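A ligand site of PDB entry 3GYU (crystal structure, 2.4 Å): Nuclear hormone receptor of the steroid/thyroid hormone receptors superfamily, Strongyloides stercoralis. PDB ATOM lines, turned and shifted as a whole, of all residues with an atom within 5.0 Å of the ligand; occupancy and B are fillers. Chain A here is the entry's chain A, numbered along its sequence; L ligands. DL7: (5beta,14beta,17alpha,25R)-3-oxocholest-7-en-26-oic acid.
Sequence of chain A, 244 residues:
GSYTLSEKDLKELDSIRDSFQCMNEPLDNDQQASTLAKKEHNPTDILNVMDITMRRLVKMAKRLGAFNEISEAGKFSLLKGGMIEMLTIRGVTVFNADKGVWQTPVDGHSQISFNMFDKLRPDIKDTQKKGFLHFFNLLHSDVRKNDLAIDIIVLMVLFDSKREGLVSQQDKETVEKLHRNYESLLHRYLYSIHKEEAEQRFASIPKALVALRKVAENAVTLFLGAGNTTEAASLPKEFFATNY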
ATOM      1  N   LEU A  36      -7.210   2.158   8.358  1.00  0.00           N
ATOM      2  CA  LEU A  36      -7.182   0.707   8.338  1.00  0.00           C
ATOM      3  C   LEU A  36      -8.533  -0.011   8.529  1.00  0.00           C
ATOM      4  O   LEU A  36      -8.876  -0.852   7.720  1.00  0.00           O
ATOM      5  CB  LEU A  36      -6.267   0.230   9.413  1.00  0.00           C
ATOM      6  CG  LEU A  36      -4.901   0.895   9.392  1.00  0.00           C
ATOM      7  CD1 LEU A  36      -4.139   0.552  10.643  1.00  0.00           C
ATOM      8  CD2 LEU A  36      -4.137   0.422   8.181  1.00  0.00           C
ATOM      9  N   ILE A  46      -5.043   3.733   0.228  1.00  0.00           N
ATOM     10  CA  ILE A  46      -3.846   2.896   0.134  1.00  0.00           C
ATOM     11  C   ILE A  46      -2.572   3.685   0.365  1.00  0.00           C
ATOM     12  O   ILE A  46      -1.634   3.161   0.943  1.00  0.00           O
ATOM     13  CB  ILE A  46      -3.702   2.270  -1.217  1.00  0.00           C
ATOM     14  CG1 ILE A  46      -4.896   1.389  -1.554  1.00  0.00           C
ATOM     15  CG2 ILE A  46      -2.456   1.513  -1.250  1.00  0.00           C
ATOM     16  CD1 ILE A  46      -5.195   0.338  -0.530  1.00  0.00           C
ATOM     17  N   VAL A  49      -2.280   4.230   4.126  1.00  0.00           N
ATOM     18  CA  VAL A  49      -1.840   3.032   4.801  1.00  0.00           C
ATOM     19  C   VAL A  49      -0.294   2.866   4.628  1.00  0.00           C
ATOM     20  O   VAL A  49       0.364   2.582   5.627  1.00  0.00           O
ATOM     21  CB  VAL A  49      -2.507   1.800   4.239  1.00  0.00           C
ATOM     22  CG1 VAL A  49      -1.815   0.531   4.741  1.00  0.00           C
ATOM     23  CG2 VAL A  49      -4.038   1.785   4.546  1.00  0.00           C
ATOM     24  N   MET A  50       0.236   3.068   3.413  1.00  0.00           N
ATOM     25  CA  MET A  50       1.652   2.980   3.162  1.00  0.00           C
ATOM     26  C   MET A  50       2.461   3.895   4.017  1.00  0.00           C
ATOM     27  O   MET A  50       3.559   3.519   4.505  1.00  0.00           O
ATOM     28  CB  MET A  50       1.979   3.329   1.727  1.00  0.00           C
ATOM     29  CG  MET A  50       1.453   2.253   0.820  1.00  0.00           C
ATOM     30  SD  MET A  50       1.940   2.505  -1.020  1.00  0.00           S
ATOM     31  CE  MET A  50       3.349   1.180  -1.248  1.00  0.00           C
ATOM     32  N   ILE A  52       1.981   4.682   7.009  1.00  0.00           N
ATOM     33  CA  ILE A  52       2.158   4.028   8.303  1.00  0.00           C
ATOM     34  C   ILE A  52       3.386   3.077   8.327  1.00  0.00           C
ATOM     35  O   ILE A  52       4.273   3.217   9.131  1.00  0.00           O
ATOM     36  CB  ILE A  52       0.977   3.154   8.676  1.00  0.00           C
ATOM     37  CG1 ILE A  52      -0.402   3.778   8.401  1.00  0.00           C
ATOM     38  CG2 ILE A  52       1.053   2.791  10.106  1.00  0.00           C
ATOM     39  CD1 ILE A  52      -0.556   5.134   9.017  1.00  0.00           C
ATOM     40  N   THR A  53       3.427   2.130   7.405  1.00  0.00           N
ATOM     41  CA  THR A  53       4.518   1.241   7.308  1.00  0.00           C
ATOM     42  C   THR A  53       5.817   1.989   6.991  1.00  0.00           C
ATOM     43  O   THR A  53       6.886   1.619   7.501  1.00  0.00           O
ATOM     44  CB  THR A  53       4.239   0.198   6.215  1.00  0.00           C
ATOM     45  OG1 THR A  53       3.026  -0.483   6.519  1.00  0.00           O
ATOM     46  CG2 THR A  53       5.369  -0.865   6.137  1.00  0.00           C
ATOM     47  N   ILE A  84      10.368   0.884  -1.340  1.00  0.00           N
ATOM     48  CA  ILE A  84       9.268   0.077  -1.944  1.00  0.00           C
ATOM     49  C   ILE A  84       9.546  -1.414  -1.820  1.00  0.00           C
ATOM     50  O   ILE A  84       8.669  -2.210  -1.667  1.00  0.00           O
ATOM     51  CB  ILE A  84       9.080   0.374  -3.436  1.00  0.00           C
ATOM     52  CG1 ILE A  84       9.047   1.883  -3.684  1.00  0.00           C
ATOM     53  CG2 ILE A  84       7.810  -0.284  -3.957  1.00  0.00           C
ATOM     54  CD1 ILE A  84       7.937   2.459  -3.073  1.00  0.00           C
ATOM     55  N   LEU A  87       8.653  -2.273   1.797  1.00  0.00           N
ATOM     56  CA  LEU A  87       7.200  -2.348   1.868  1.00  0.00           C
ATOM     57  C   LEU A  87       6.695  -3.651   1.316  1.00  0.00           C
ATOM     58  O   LEU A  87       5.855  -4.265   1.900  1.00  0.00           O
ATOM     59  CB  LEU A  87       6.536  -1.191   1.129  1.00  0.00           C
ATOM     60  CG  LEU A  87       6.462   0.128   1.866  1.00  0.00           C
ATOM     61  CD1 LEU A  87       5.932   1.145   0.863  1.00  0.00           C
ATOM     62  CD2 LEU A  87       5.456   0.050   3.142  1.00  0.00           C
ATOM     63  N   THR A  88       7.224  -4.066   0.155  1.00  0.00           N
ATOM     64  CA  THR A  88       6.718  -5.220  -0.538  1.00  0.00           C
ATOM     65  C   THR A  88       6.982  -6.450   0.307  1.00  0.00           C
ATOM     66  O   THR A  88       6.142  -7.309   0.380  1.00  0.00           O
ATOM     67  CB  THR A  88       7.349  -5.326  -1.886  1.00  0.00           C
ATOM     68  OG1 THR A  88       7.068  -4.130  -2.631  1.00  0.00           O
ATOM     69  CG2 THR A  88       6.829  -6.566  -2.618  1.00  0.00           C
ATOM     70  N   ARG A  90       7.287  -6.486   3.472  1.00  0.00           N
ATOM     71  CA  ARG A  90       6.333  -6.405   4.550  1.00  0.00           C
ATOM     72  C   ARG A  90       4.977  -6.896   4.096  1.00  0.00           C
ATOM     73  O   ARG A  90       4.161  -7.422   4.870  1.00  0.00           O
ATOM     74  CB  ARG A  90       6.247  -4.991   5.023  1.00  0.00           C
ATOM     75  CG  ARG A  90       5.066  -4.781   5.933  1.00  0.00           C
ATOM     76  CD  ARG A  90       5.239  -5.368   7.378  1.00  0.00           C
ATOM     77  NE  ARG A  90       4.194  -4.862   8.315  1.00  0.00           N
ATOM     78  CZ  ARG A  90       4.099  -5.237   9.587  1.00  0.00           C
ATOM     79  NH1 ARG A  90       4.971  -6.063  10.116  1.00  0.00           N
ATOM     80  NH2 ARG A  90       3.117  -4.794  10.323  1.00  0.00           N
ATOM     81  N   GLY A  91       4.732  -6.688   2.796  1.00  0.00           N
ATOM     82  CA  GLY A  91       3.489  -7.102   2.179  1.00  0.00           C
ATOM     83  C   GLY A  91       3.371  -8.634   2.036  1.00  0.00           C
ATOM     84  O   GLY A  91       2.292  -9.210   2.174  1.00  0.00           O
ATOM     85  N   VAL A  94       2.560 -10.189   5.756  1.00  0.00           N
ATOM     86  CA  VAL A  94       1.226 -10.103   6.317  1.00  0.00           C
ATOM     87  C   VAL A  94       0.145 -10.485   5.314  1.00  0.00           C
ATOM     88  O   VAL A  94      -1.021 -10.286   5.549  1.00  0.00           O
ATOM     89  CB  VAL A  94       0.926  -8.718   6.849  1.00  0.00           C
ATOM     90  CG1 VAL A  94       2.096  -8.258   7.794  1.00  0.00           C
ATOM     91  CG2 VAL A  94       0.698  -7.763   5.711  1.00  0.00           C
ATOM     92  N   TRP A 102      -4.503  -8.456   2.935  1.00  0.00           N
ATOM     93  CA  TRP A 102      -3.419  -8.234   3.800  1.00  0.00           C
ATOM     94  C   TRP A 102      -3.979  -8.067   5.185  1.00  0.00           C
ATOM     95  O   TRP A 102      -4.847  -7.230   5.377  1.00  0.00           O
ATOM     96  CB  TRP A 102      -2.684  -6.936   3.402  1.00  0.00           C
ATOM     97  CG  TRP A 102      -1.846  -7.024   2.191  1.00  0.00           C
ATOM     98  CD1 TRP A 102      -0.632  -7.573   2.103  1.00  0.00           C
ATOM     99  CD2 TRP A 102      -2.144  -6.527   0.877  1.00  0.00           C
ATOM    100  NE1 TRP A 102      -0.129  -7.465   0.842  1.00  0.00           N
ATOM    101  CE2 TRP A 102      -1.066  -6.843   0.059  1.00  0.00           C
ATOM    102  CE3 TRP A 102      -3.222  -5.831   0.311  1.00  0.00           C
ATOM    103  CZ2 TRP A 102      -1.012  -6.464  -1.249  1.00  0.00           C
ATOM    104  CZ3 TRP A 102      -3.167  -5.492  -1.012  1.00  0.00           C
ATOM    105  CH2 TRP A 102      -2.077  -5.813  -1.778  1.00  0.00           C
ATOM    106  N   THR A 104      -2.952  -6.987   8.925  1.00  0.00           N
ATOM    107  CA  THR A 104      -1.927  -6.462   9.761  1.00  0.00           C
ATOM    108  C   THR A 104      -2.036  -6.933  11.220  1.00  0.00           C
ATOM    109  O   THR A 104      -3.110  -6.913  11.801  1.00  0.00           O
ATOM    110  CB  THR A 104      -1.994  -4.948   9.722  1.00  0.00           C
ATOM    111  OG1 THR A 104      -1.093  -4.421  10.675  1.00  0.00           O
ATOM    112  CG2 THR A 104      -3.386  -4.482  10.011  1.00  0.00           C
ATOM    113  N   VAL A 106      -0.971  -5.369  13.744  1.00  0.00           N
ATOM    114  CA  VAL A 106      -1.179  -4.244  14.625  1.00  0.00           C
ATOM    115  C   VAL A 106      -2.638  -3.880  14.786  1.00  0.00           C
ATOM    116  O   VAL A 106      -2.970  -3.102  15.652  1.00  0.00           O
ATOM    117  CB  VAL A 106      -0.449  -3.020  14.097  1.00  0.00           C
ATOM    118  CG1 VAL A 106       0.936  -3.440  13.604  1.00  0.00           C
ATOM    119  CG2 VAL A 106      -1.225  -2.354  12.976  1.00  0.00           C
ATOM    120  N   ILE A 112      -7.089  -5.667   3.923  1.00  0.00           N
ATOM    121  CA  ILE A 112      -6.927  -4.900   2.703  1.00  0.00           C
ATOM    122  C   ILE A 112      -6.967  -5.749   1.498  1.00  0.00           C
ATOM    123  O   ILE A 112      -6.105  -6.538   1.281  1.00  0.00           O
ATOM    124  CB  ILE A 112      -5.618  -4.131   2.713  1.00  0.00           C
ATOM    125  CG1 ILE A 112      -5.664  -3.077   3.802  1.00  0.00           C
ATOM    126  CG2 ILE A 112      -5.398  -3.453   1.400  1.00  0.00           C
ATOM    127  CD1 ILE A 112      -4.486  -2.416   3.919  1.00  0.00           C
ATOM    128  N   MET A 116      -7.434  -4.157  -4.659  1.00  0.00           N
ATOM    129  CA  MET A 116      -7.297  -2.745  -4.713  1.00  0.00           C
ATOM    130  C   MET A 116      -6.411  -2.390  -5.931  1.00  0.00           C
ATOM    131  O   MET A 116      -6.456  -1.224  -6.345  1.00  0.00           O
ATOM    132  CB  MET A 116      -6.676  -2.186  -3.406  1.00  0.00           C
ATOM    133  CG  MET A 116      -5.228  -2.741  -3.086  1.00  0.00           C
ATOM    134  SD  MET A 116      -3.717  -1.739  -3.952  1.00  0.00           S
ATOM    135  CE  MET A 116      -2.260  -3.120  -3.946  1.00  0.00           C
ATOM    136  N   PHE A 117      -5.597  -3.305  -6.446  1.00  0.00           N
ATOM    137  CA  PHE A 117      -4.817  -3.039  -7.699  1.00  0.00           C
ATOM    138  C   PHE A 117      -5.730  -2.650  -8.870  1.00  0.00           C
ATOM    139  O   PHE A 117      -5.302  -1.942  -9.802  1.00  0.00           O
ATOM    140  CB  PHE A 117      -4.051  -4.262  -8.165  1.00  0.00           C
ATOM    141  CG  PHE A 117      -2.760  -4.496  -7.471  1.00  0.00           C
ATOM    142  CD1 PHE A 117      -2.689  -5.470  -6.496  1.00  0.00           C
ATOM    143  CD2 PHE A 117      -1.594  -3.857  -7.879  1.00  0.00           C
ATOM    144  CE1 PHE A 117      -1.488  -5.731  -5.895  1.00  0.00           C
ATOM    145  CE2 PHE A 117      -0.392  -4.148  -7.304  1.00  0.00           C
ATOM    146  CZ  PHE A 117      -0.321  -5.075  -6.307  1.00  0.00           C
ATOM    147  N   GLN A 128       1.517  -6.024 -12.125  1.00  0.00           N
ATOM    148  CA  GLN A 128       1.962  -5.861 -10.777  1.00  0.00           C
ATOM    149  C   GLN A 128       1.292  -6.837  -9.862  1.00  0.00           C
ATOM    150  O   GLN A 128       1.842  -7.221  -8.871  1.00  0.00           O
ATOM    151  CB  GLN A 128       1.671  -4.458 -10.294  1.00  0.00           C
ATOM    152  CG  GLN A 128       2.475  -3.425 -10.966  1.00  0.00           C
ATOM    153  CD  GLN A 128       3.941  -3.723 -10.882  1.00  0.00           C
ATOM    154  OE1 GLN A 128       4.514  -4.109 -11.876  1.00  0.00           O
ATOM    155  NE2 GLN A 128       4.547  -3.562  -9.696  1.00  0.00           N
ATOM    156  N   PHE A 132       3.545  -9.574  -7.815  1.00  0.00           N
ATOM    157  CA  PHE A 132       3.511  -9.625  -6.381  1.00  0.00           C
ATOM    158  C   PHE A 132       3.304 -11.060  -5.920  1.00  0.00           C
ATOM    159  O   PHE A 132       4.013 -11.517  -5.041  1.00  0.00           O
ATOM    160  CB  PHE A 132       2.411  -8.764  -5.794  1.00  0.00           C
ATOM    161  CG  PHE A 132       2.296  -8.899  -4.296  1.00  0.00           C
ATOM    162  CD1 PHE A 132       3.161  -8.195  -3.472  1.00  0.00           C
ATOM    163  CD2 PHE A 132       1.390  -9.756  -3.692  1.00  0.00           C
ATOM    164  CE1 PHE A 132       3.107  -8.311  -2.086  1.00  0.00           C
ATOM    165  CE2 PHE A 132       1.371  -9.911  -2.291  1.00  0.00           C
ATOM    166  CZ  PHE A 132       2.194  -9.154  -1.498  1.00  0.00           C
ATOM    167  N   VAL A 215       9.656  -6.313  -9.300  1.00  0.00           N
ATOM    168  CA  VAL A 215       8.288  -5.908  -8.894  1.00  0.00           C
ATOM    169  C   VAL A 215       8.156  -4.514  -8.291  1.00  0.00           C
ATOM    170  O   VAL A 215       7.216  -3.727  -8.716  1.00  0.00           O
ATOM    171  CB  VAL A 215       7.687  -6.874  -7.913  1.00  0.00           C
ATOM    172  CG1 VAL A 215       6.349  -6.457  -7.552  1.00  0.00           C
ATOM    173  CG2 VAL A 215       7.547  -8.197  -8.588  1.00  0.00           C
ATOM    174  N   ALA A 219       6.591  -0.222  -9.890  1.00  0.00           N
ATOM    175  CA  ALA A 219       5.463   0.010  -9.081  1.00  0.00           C
ATOM    176  C   ALA A 219       5.233   1.505  -8.918  1.00  0.00           C
ATOM    177  O   ALA A 219       4.114   1.923  -8.538  1.00  0.00           O
ATOM    178  CB  ALA A 219       5.610  -0.608  -7.738  1.00  0.00           C
ATOM    179  N   LEU A 222       2.198   3.384 -10.479  1.00  0.00           N
ATOM    180  CA  LEU A 222       0.903   2.726 -10.251  1.00  0.00           C
ATOM    181  C   LEU A 222      -0.264   3.696  -9.975  1.00  0.00           C
ATOM    182  O   LEU A 222      -1.430   3.289 -10.124  1.00  0.00           O
ATOM    183  CB  LEU A 222       0.981   1.693  -9.102  1.00  0.00           C
ATOM    184  CG  LEU A 222       1.135   0.247  -9.507  1.00  0.00           C
ATOM    185  CD1 LEU A 222       1.369  -0.543  -8.253  1.00  0.00           C
ATOM    186  CD2 LEU A 222      -0.053  -0.258 -10.322  1.00  0.00           C
ATOM    187  N   PHE A 240       5.781   7.475  -5.183  1.00  0.00           N
ATOM    188  CA  PHE A 240       4.799   7.143  -6.195  1.00  0.00           C
ATOM    189  C   PHE A 240       4.407   8.378  -7.004  1.00  0.00           C
ATOM    190  O   PHE A 240       3.960   9.320  -6.450  1.00  0.00           O
ATOM    191  CB  PHE A 240       3.596   6.456  -5.549  1.00  0.00           C
ATOM    192  CG  PHE A 240       3.890   5.058  -5.044  1.00  0.00           C
ATOM    193  CD1 PHE A 240       3.886   3.990  -5.904  1.00  0.00           C
ATOM    194  CD2 PHE A 240       4.205   4.840  -3.731  1.00  0.00           C
ATOM    195  CE1 PHE A 240       4.169   2.722  -5.456  1.00  0.00           C
ATOM    196  CE2 PHE A 240       4.481   3.565  -3.261  1.00  0.00           C
ATOM    197  CZ  PHE A 240       4.476   2.505  -4.115  1.00  0.00           C
HETATM  198  O3  DL7 L   1       1.235  -3.049   8.956  1.00  0.00           O
HETATM  199  C27 DL7 L   1       0.973  -1.847   8.677  1.00  0.00           C
HETATM  200  O2  DL7 L   1       1.778  -0.912   8.837  1.00  0.00           O
HETATM  201  C25 DL7 L   1      -0.366  -1.447   8.218  1.00  0.00           C
HETATM  202  C26 DL7 L   1      -1.269  -1.455   9.446  1.00  0.00           C
HETATM  203  C24 DL7 L   1      -0.837  -2.449   7.180  1.00  0.00           C
HETATM  204  C23 DL7 L   1       0.120  -2.489   6.025  1.00  0.00           C
HETATM  205  C22 DL7 L   1      -0.278  -3.477   4.927  1.00  0.00           C
HETATM  206  C20 DL7 L   1       0.772  -3.240   3.819  1.00  0.00           C
HETATM  207  C21 DL7 L   1       1.946  -4.183   4.184  1.00  0.00           C
HETATM  208  C17 DL7 L   1       0.225  -3.339   2.363  1.00  0.00           C
HETATM  209  C16 DL7 L   1      -0.951  -2.410   2.061  1.00  0.00           C
HETATM  210  C15 DL7 L   1      -0.877  -1.896   0.628  1.00  0.00           C
HETATM  211  C14 DL7 L   1       0.208  -2.822   0.039  1.00  0.00           C
HETATM  212  C8  DL7 L   1       0.905  -2.486  -1.251  1.00  0.00           C
HETATM  213  C7  DL7 L   1       0.674  -1.507  -2.097  1.00  0.00           C
HETATM  214  C6  DL7 L   1       1.225  -1.009  -3.393  1.00  0.00           C
HETATM  215  C13 DL7 L   1       1.195  -3.027   1.167  1.00  0.00           C
HETATM  216  C18 DL7 L   1       1.939  -1.671   1.344  1.00  0.00           C
HETATM  217  C12 DL7 L   1       2.088  -4.181   0.747  1.00  0.00           C
HETATM  218  C11 DL7 L   1       2.862  -3.939  -0.555  1.00  0.00           C
HETATM  219  C9  DL7 L   1       2.000  -3.432  -1.724  1.00  0.00           C
HETATM  220  C10 DL7 L   1       2.853  -2.978  -2.980  1.00  0.00           C
HETATM  221  C1  DL7 L   1       3.465  -4.189  -3.676  1.00  0.00           C
HETATM  222  C19 DL7 L   1       3.959  -2.033  -2.536  1.00  0.00           C
HETATM  223  C5  DL7 L   1       1.932  -2.279  -4.005  1.00  0.00           C
HETATM  224  C4  DL7 L   1       2.587  -1.925  -5.317  1.00  0.00           C
HETATM  225  C3  DL7 L   1       3.338  -3.064  -5.927  1.00  0.00           C
HETATM  226  O1  DL7 L   1       3.247  -3.363  -7.126  1.00  0.00           O
HETATM  227  C2  DL7 L   1       4.161  -3.878  -4.969  1.00  0.00           C
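Leu 36 touches the ligand.
CG1 of Val 49 touches C23 of the ligand, at 3.8 Å.
Met 50 touches the ligand (CE to C19, 3.5 Å).
CG2 of Ile 52 touches O2 of the ligand, at 3.98 Å.
Leu 87 touches the ligand (O to C11, 3.9 Å).
OG1 of Thr 88 touches C2 of the ligand, 3.7 Å away.
CA of Gly 91 touches C12 of the ligand (3.5 Å).
Trp 102 touches the ligand (NE1 to C12, 3.96 Å).
CG2 of Val 106 touches C26 of the ligand, at 3.6 Å.
Ile 112 touches the ligand (CD1 to C16, 3.99 Å).
CE of Met 116 touches C7 of the ligand, 3.8 Å away.
Phe 117 touches the ligand.
Ala 219 touches the ligand.
Leu 222 touches the ligand (CD1 to C4, 3.5 Å).
Hydrophobic or aromatic side chains within 4 Å of the ligand: Leu 36, Val 49, Met 50, Ile 52, Val 106, Ile 112, Met 116, Phe 117, Ala 219 and Leu 222.
Along chain A the residues within 4 Å of the ligand span positions 36 to 222.
O2 of the ligand is in hydrogen-bond range of OG1 of Thr 53 (2.7 Å).
An oxygen (O1) of the ligand sits at hydrogen-bond distance from the side-chain amide nitrogen of Gln 128 (2.9 Å).
An oxygen (O3) of the ligand is in salt-bridge range of the guanidinium group (NH2) of Arg 90, 2.9 Å away.
O3 of the ligand sits at hydrogen-bond distance from OG1 of Thr 104.
The backbone carbonyl oxygen (O) of Val 215 sits at hydrogen-bond distance from the side-chain amide nitrogen (NE2) of Gln 128 (2.8 Å).
The side-chain hydroxyl (OG1) of Thr 104 sits close to the backbone NH (N) of Val 106, 3.2 Å away.
The indole nitrogen (NE1) of Trp 102 is in hydrogen-bond range of the backbone carbonyl oxygen (O) of Gly 91 (3.3 Å).
The side-chain hydroxyl of Thr 88 is in hydrogen-bond range of the backbone carbonyl oxygen of Ile 84, 2.7 Å away.
N of Trp 102 sits at hydrogen-bond distance from O of Ile 112 (3.0 Å).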
